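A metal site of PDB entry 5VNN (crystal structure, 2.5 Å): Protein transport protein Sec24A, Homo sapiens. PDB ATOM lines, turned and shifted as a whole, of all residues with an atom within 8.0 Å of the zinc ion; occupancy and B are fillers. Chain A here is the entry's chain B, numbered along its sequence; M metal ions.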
ATOM      1  N   ARG A  85       7.905 -17.114  19.079  1.00  0.00           N
ATOM      2  CA  ARG A  85       6.505 -17.402  19.358  1.00  0.00           C
ATOM      3  C   ARG A  85       6.318 -18.900  19.467  1.00  0.00           C
ATOM      4  O   ARG A  85       6.869 -19.659  18.667  1.00  0.00           O
ATOM      5  CB  ARG A  85       5.588 -16.828  18.272  1.00  0.00           C
ATOM      6  CG  ARG A  85       5.764 -15.346  18.029  1.00  0.00           C
ATOM      7  CD  ARG A  85       4.790 -14.845  16.985  1.00  0.00           C
ATOM      8  NE  ARG A  85       3.407 -14.889  17.460  1.00  0.00           N
ATOM      9  CZ  ARG A  85       2.363 -14.484  16.754  1.00  0.00           C
ATOM     10  NH1 ARG A  85       2.537 -13.994  15.527  1.00  0.00           N
ATOM     11  NH2 ARG A  85       1.141 -14.564  17.253  1.00  0.00           N
ATOM     12  N   CYS A  86       5.535 -19.326  20.469  1.00  0.00           N
ATOM     13  CA  CYS A  86       5.246 -20.749  20.653  1.00  0.00           C
ATOM     14  C   CYS A  86       4.683 -21.352  19.380  1.00  0.00           C
ATOM     15  O   CYS A  86       3.790 -20.779  18.748  1.00  0.00           O
ATOM     16  CB  CYS A  86       4.252 -20.921  21.808  1.00  0.00           C
ATOM     17  SG  CYS A  86       3.500 -22.567  21.910  1.00  0.00           S
ATOM     18  N   ARG A  87       5.215 -22.509  18.989  1.00  0.00           N
ATOM     19  CA  ARG A  87       4.892 -23.115  17.698  1.00  0.00           C
ATOM     20  C   ARG A  87       3.441 -23.542  17.586  1.00  0.00           C
ATOM     21  O   ARG A  87       2.972 -23.789  16.462  1.00  0.00           O
ATOM     22  CB  ARG A  87       5.805 -24.313  17.445  1.00  0.00           C
ATOM     23  CG  ARG A  87       7.276 -23.947  17.250  1.00  0.00           C
ATOM     24  CD  ARG A  87       8.106 -25.183  16.964  1.00  0.00           C
ATOM     25  NE  ARG A  87       9.521 -24.863  16.796  1.00  0.00           N
ATOM     26  CZ  ARG A  87      10.460 -25.744  16.497  1.00  0.00           C
ATOM     27  NH1 ARG A  87      10.138 -27.023  16.332  1.00  0.00           N
ATOM     28  NH2 ARG A  87      11.730 -25.366  16.368  1.00  0.00           N
ATOM     29  N   SER A  88       2.701 -23.641  18.690  1.00  0.00           N
ATOM     30  CA  SER A  88       1.313 -24.100  18.672  1.00  0.00           C
ATOM     31  C   SER A  88       0.325 -22.945  18.760  1.00  0.00           C
ATOM     32  O   SER A  88      -0.418 -22.692  17.797  1.00  0.00           O
ATOM     33  CB  SER A  88       1.071 -25.098  19.807  1.00  0.00           C
ATOM     34  OG  SER A  88       1.711 -26.339  19.552  1.00  0.00           O
ATOM     35  N   CYS A  89       0.280 -22.232  19.883  1.00  0.00           N
ATOM     36  CA  CYS A  89      -0.690 -21.174  20.098  1.00  0.00           C
ATOM     37  C   CYS A  89      -0.165 -19.786  19.734  1.00  0.00           C
ATOM     38  O   CYS A  89      -0.904 -18.799  19.892  1.00  0.00           O
ATOM     39  CB  CYS A  89      -1.164 -21.161  21.555  1.00  0.00           C
ATOM     40  SG  CYS A  89       0.101 -20.597  22.715  1.00  0.00           S
ATOM     41  N   ARG A  90       1.071 -19.690  19.267  1.00  0.00           N
ATOM     42  CA  ARG A  90       1.695 -18.442  18.807  1.00  0.00           C
ATOM     43  C   ARG A  90       1.863 -17.415  19.917  1.00  0.00           C
ATOM     44  O   ARG A  90       1.907 -16.206  19.635  1.00  0.00           O
ATOM     45  CB  ARG A  90       0.919 -17.834  17.631  1.00  0.00           C
ATOM     46  CG  ARG A  90       0.689 -18.773  16.459  1.00  0.00           C
ATOM     47  CD  ARG A  90       1.970 -19.479  16.056  1.00  0.00           C
ATOM     48  NE  ARG A  90       3.079 -18.557  15.845  1.00  0.00           N
ATOM     49  CZ  ARG A  90       3.400 -18.003  14.680  1.00  0.00           C
ATOM     50  NH1 ARG A  90       2.689 -18.295  13.593  1.00  0.00           N
ATOM     51  NH2 ARG A  90       4.424 -17.169  14.593  1.00  0.00           N
ATOM     52  N   THR A  91       1.959 -17.849  21.164  1.00  0.00           N
ATOM     53  CA  THR A  91       2.206 -16.925  22.260  1.00  0.00           C
ATOM     54  C   THR A  91       3.629 -16.400  22.200  1.00  0.00           C
ATOM     55  O   THR A  91       4.574 -17.163  21.983  1.00  0.00           O
ATOM     56  CB  THR A  91       1.943 -17.606  23.609  1.00  0.00           C
ATOM     57  OG1 THR A  91       0.609 -18.127  23.637  1.00  0.00           O
ATOM     58  CG2 THR A  91       2.126 -16.612  24.750  1.00  0.00           C
ATOM     59  N   TYR A  92       3.787 -15.094  22.405  1.00  0.00           N
ATOM     60  CA  TYR A  92       5.115 -14.491  22.381  1.00  0.00           C
ATOM     61  C   TYR A  92       5.891 -14.847  23.643  1.00  0.00           C
ATOM     62  O   TYR A  92       5.316 -15.043  24.720  1.00  0.00           O
ATOM     63  CB  TYR A  92       5.001 -12.979  22.243  1.00  0.00           C
ATOM     64  CG  TYR A  92       4.466 -12.547  20.896  1.00  0.00           C
ATOM     65  CD1 TYR A  92       3.100 -12.546  20.624  1.00  0.00           C
ATOM     66  CD2 TYR A  92       5.334 -12.142  19.886  1.00  0.00           C
ATOM     67  CE1 TYR A  92       2.614 -12.152  19.390  1.00  0.00           C
ATOM     68  CE2 TYR A  92       4.858 -11.748  18.654  1.00  0.00           C
ATOM     69  CZ  TYR A  92       3.496 -11.751  18.415  1.00  0.00           C
ATOM     70  OH  TYR A  92       3.041 -11.358  17.178  1.00  0.00           O
ATOM     71  N   ASN A  94       7.444 -14.620  26.838  1.00  0.00           N
ATOM     72  CA  ASN A  94       7.140 -13.702  27.924  1.00  0.00           C
ATOM     73  C   ASN A  94       7.918 -14.089  29.182  1.00  0.00           C
ATOM     74  O   ASN A  94       8.420 -15.208  29.289  1.00  0.00           O
ATOM     75  CB  ASN A  94       5.633 -13.684  28.202  1.00  0.00           C
ATOM     76  CG  ASN A  94       5.085 -15.060  28.527  1.00  0.00           C
ATOM     77  OD1 ASN A  94       4.992 -15.440  29.689  1.00  0.00           O
ATOM     78  ND2 ASN A  94       4.711 -15.806  27.502  1.00  0.00           N
ATOM     79  N   TRP A 105      12.117 -24.058  26.082  1.00  0.00           N
ATOM     80  CA  TRP A 105      11.264 -23.318  27.004  1.00  0.00           C
ATOM     81  C   TRP A 105       9.829 -23.789  26.873  1.00  0.00           C
ATOM     82  O   TRP A 105       9.349 -24.064  25.762  1.00  0.00           O
ATOM     83  CB  TRP A 105      11.355 -21.805  26.767  1.00  0.00           C
ATOM     84  CG  TRP A 105      10.915 -21.374  25.410  1.00  0.00           C
ATOM     85  CD1 TRP A 105      11.651 -21.406  24.258  1.00  0.00           C
ATOM     86  CD2 TRP A 105       9.635 -20.830  25.050  1.00  0.00           C
ATOM     87  NE1 TRP A 105      10.905 -20.916  23.206  1.00  0.00           N
ATOM     88  CE2 TRP A 105       9.669 -20.555  23.666  1.00  0.00           C
ATOM     89  CE3 TRP A 105       8.470 -20.541  25.761  1.00  0.00           C
ATOM     90  CZ2 TRP A 105       8.582 -20.013  22.986  1.00  0.00           C
ATOM     91  CZ3 TRP A 105       7.384 -20.008  25.082  1.00  0.00           C
ATOM     92  CH2 TRP A 105       7.448 -19.752  23.708  1.00  0.00           C
ATOM     93  N   LYS A 106       9.134 -23.873  28.005  1.00  0.00           N
ATOM     94  CA  LYS A 106       7.742 -24.300  28.043  1.00  0.00           C
ATOM     95  C   LYS A 106       6.821 -23.098  27.959  1.00  0.00           C
ATOM     96  O   LYS A 106       6.989 -22.123  28.703  1.00  0.00           O
ATOM     97  CB  LYS A 106       7.460 -25.098  29.317  1.00  0.00           C
ATOM     98  CG  LYS A 106       5.973 -25.293  29.600  1.00  0.00           C
ATOM     99  CD  LYS A 106       5.723 -26.150  30.831  1.00  0.00           C
ATOM    100  CE  LYS A 106       5.886 -27.630  30.514  1.00  0.00           C
ATOM    101  NZ  LYS A 106       5.575 -28.486  31.699  1.00  0.00           N
ATOM    102  N   CYS A 107       5.843 -23.160  27.058  1.00  0.00           N
ATOM    103  CA  CYS A 107       4.881 -22.074  26.904  1.00  0.00           C
ATOM    104  C   CYS A 107       3.957 -22.011  28.111  1.00  0.00           C
ATOM    105  O   CYS A 107       3.409 -23.028  28.543  1.00  0.00           O
ATOM    106  CB  CYS A 107       4.076 -22.273  25.620  1.00  0.00           C
ATOM    107  SG  CYS A 107       2.875 -20.967  25.242  1.00  0.00           S
ATOM    108  N   ASN A 108       3.786 -20.819  28.671  1.00  0.00           N
ATOM    109  CA  ASN A 108       2.946 -20.650  29.845  1.00  0.00           C
ATOM    110  C   ASN A 108       1.463 -20.577  29.533  1.00  0.00           C
ATOM    111  O   ASN A 108       0.658 -20.358  30.444  1.00  0.00           O
ATOM    112  CB  ASN A 108       3.370 -19.401  30.625  1.00  0.00           C
ATOM    113  CG  ASN A 108       3.398 -18.157  29.757  1.00  0.00           C
ATOM    114  OD1 ASN A 108       3.445 -18.248  28.533  1.00  0.00           O
ATOM    115  ND2 ASN A 108       3.365 -16.999  30.398  1.00  0.00           N
ATOM    116  N   LEU A 109       1.073 -20.750  28.266  1.00  0.00           N
ATOM    117  CA  LEU A 109      -0.329 -20.683  27.868  1.00  0.00           C
ATOM    118  C   LEU A 109      -0.859 -22.000  27.308  1.00  0.00           C
ATOM    119  O   LEU A 109      -2.015 -22.343  27.561  1.00  0.00           O
ATOM    120  CB  LEU A 109      -0.534 -19.576  26.829  1.00  0.00           C
ATOM    121  CG  LEU A 109      -0.853 -18.185  27.368  1.00  0.00           C
ATOM    122  CD1 LEU A 109       0.293 -17.628  28.189  1.00  0.00           C
ATOM    123  CD2 LEU A 109      -1.169 -17.252  26.222  1.00  0.00           C
ATOM    124  N   CYS A 110      -0.053 -22.748  26.555  1.00  0.00           N
ATOM    125  CA  CYS A 110      -0.475 -24.043  26.056  1.00  0.00           C
ATOM    126  C   CYS A 110       0.519 -25.152  26.400  1.00  0.00           C
ATOM    127  O   CYS A 110       0.399 -26.266  25.883  1.00  0.00           O
ATOM    128  CB  CYS A 110      -0.698 -23.989  24.542  1.00  0.00           C
ATOM    129  SG  CYS A 110       0.791 -23.783  23.547  1.00  0.00           S
ATOM    130  N   TYR A 111       1.507 -24.876  27.251  1.00  0.00           N
ATOM    131  CA  TYR A 111       2.413 -25.849  27.871  1.00  0.00           C
ATOM    132  C   TYR A 111       3.303 -26.594  26.875  1.00  0.00           C
ATOM    133  O   TYR A 111       4.011 -27.533  27.265  1.00  0.00           O
ATOM    134  CB  TYR A 111       1.648 -26.864  28.733  1.00  0.00           C
ATOM    135  CG  TYR A 111       0.694 -26.204  29.710  1.00  0.00           C
ATOM    136  CD1 TYR A 111       1.054 -25.049  30.379  1.00  0.00           C
ATOM    137  CD2 TYR A 111      -0.572 -26.745  29.945  1.00  0.00           C
ATOM    138  CE1 TYR A 111       0.183 -24.437  31.270  1.00  0.00           C
ATOM    139  CE2 TYR A 111      -1.443 -26.143  30.838  1.00  0.00           C
ATOM    140  CZ  TYR A 111      -1.058 -24.991  31.492  1.00  0.00           C
ATOM    141  OH  TYR A 111      -1.900 -24.367  32.388  1.00  0.00           O
ATOM    142  N   ARG A 112       3.289 -26.217  25.595  1.00  0.00           N
ATOM    143  CA  ARG A 112       4.187 -26.834  24.627  1.00  0.00           C
ATOM    144  C   ARG A 112       5.616 -26.349  24.827  1.00  0.00           C
ATOM    145  O   ARG A 112       5.864 -25.178  25.122  1.00  0.00           O
ATOM    146  CB  ARG A 112       3.718 -26.541  23.197  1.00  0.00           C
ATOM    147  CG  ARG A 112       4.858 -26.471  22.191  1.00  0.00           C
ATOM    148  CD  ARG A 112       4.494 -27.134  20.870  1.00  0.00           C
ATOM    149  NE  ARG A 112       5.706 -27.536  20.151  1.00  0.00           N
ATOM    150  CZ  ARG A 112       5.738 -27.874  18.867  1.00  0.00           C
ATOM    151  NH1 ARG A 112       4.636 -27.851  18.140  1.00  0.00           N
ATOM    152  NH2 ARG A 112       6.892 -28.224  18.313  1.00  0.00           N
ATOM    153  N   VAL A 113       6.568 -27.264  24.663  1.00  0.00           N
ATOM    154  CA  VAL A 113       7.993 -26.949  24.780  1.00  0.00           C
ATOM    155  C   VAL A 113       8.508 -26.515  23.412  1.00  0.00           C
ATOM    156  O   VAL A 113       8.189 -27.140  22.387  1.00  0.00           O
ATOM    157  CB  VAL A 113       8.772 -28.162  25.325  1.00  0.00           C
ATOM    158  CG1 VAL A 113      10.180 -27.757  25.735  1.00  0.00           C
ATOM    159  CG2 VAL A 113       8.015 -28.790  26.488  1.00  0.00           C
ATOM    160  N   ASN A 114       9.310 -25.454  23.396  1.00  0.00           N
ATOM    161  CA  ASN A 114       9.831 -24.883  22.159  1.00  0.00           C
ATOM    162  C   ASN A 114      11.342 -24.746  22.248  1.00  0.00           C
ATOM    163  O   ASN A 114      11.895 -24.538  23.326  1.00  0.00           O
ATOM    164  CB  ASN A 114       9.203 -23.516  21.869  1.00  0.00           C
ATOM    165  CG  ASN A 114       7.711 -23.610  21.588  1.00  0.00           C
ATOM    166  OD1 ASN A 114       7.290 -23.639  20.431  1.00  0.00           O
ATOM    167  ND2 ASN A 114       6.917 -23.667  22.650  1.00  0.00           N
ATOM    168  N   ARG A 407      -4.905 -13.587  24.545  1.00  0.00           N
ATOM    169  CA  ARG A 407      -4.602 -14.978  24.827  1.00  0.00           C
ATOM    170  C   ARG A 407      -4.580 -15.229  26.324  1.00  0.00           C
ATOM    171  O   ARG A 407      -4.103 -14.391  27.093  1.00  0.00           O
ATOM    172  CB  ARG A 407      -3.268 -15.390  24.212  1.00  0.00           C
ATOM    173  CG  ARG A 407      -3.249 -15.477  22.697  1.00  0.00           C
ATOM    174  CD  ARG A 407      -1.963 -16.119  22.210  1.00  0.00           C
ATOM    175  NE  ARG A 407      -1.877 -16.135  20.749  1.00  0.00           N
ATOM    176  CZ  ARG A 407      -1.315 -15.174  20.029  1.00  0.00           C
ATOM    177  NH1 ARG A 407      -0.781 -14.114  20.631  1.00  0.00           N
ATOM    178  NH2 ARG A 407      -1.289 -15.263  18.715  1.00  0.00           N
HETATM  179 ZN    ZN M   1       1.905 -21.836  23.364  1.00  0.00          ZN
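The backbone NH (N) of Cys 86 is in hydrogen-bond range of the backbone carbonyl oxygen (O) of Thr 91, at 2.8 Å. The backbone NH (N) of Ser 88 lies close to the side-chain sulfur (SG) of Cys 86 (3.5 Å). The side-chain sulfur (SG) of Cys 86 sits close to the side-chain amide nitrogen (ND2) of Asn 114. The side-chain hydroxyl (OG1) of Thr 91 sits close to the side-chain sulfur (SG) of Cys 89, 2.7 Å away. The guanidinium group (NE) of Arg 407 lies within hydrogen-bond range of the backbone carbonyl oxygen (O) of Cys 89 (3.0 Å). SG of Cys 107 lies close to N of Leu 109 (3.5 Å). The backbone NH (N) of Cys 107 sits at hydrogen-bond distance from the backbone carbonyl oxygen (O) of Arg 112, at 2.8 Å.
The zinc ion is bound by SG of Cys 110, 2.3 Å away. The zinc ion is bound by SG of Cys 86, at 2.3 Å. The zinc ion is bound by SG of Cys 89 (2.3 Å). The zinc ion is bound by SG of Cys 107.
Thr 91 touches the zinc ion. Of the 20 residues printed, 5 come within 4 Å of the zinc ion.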
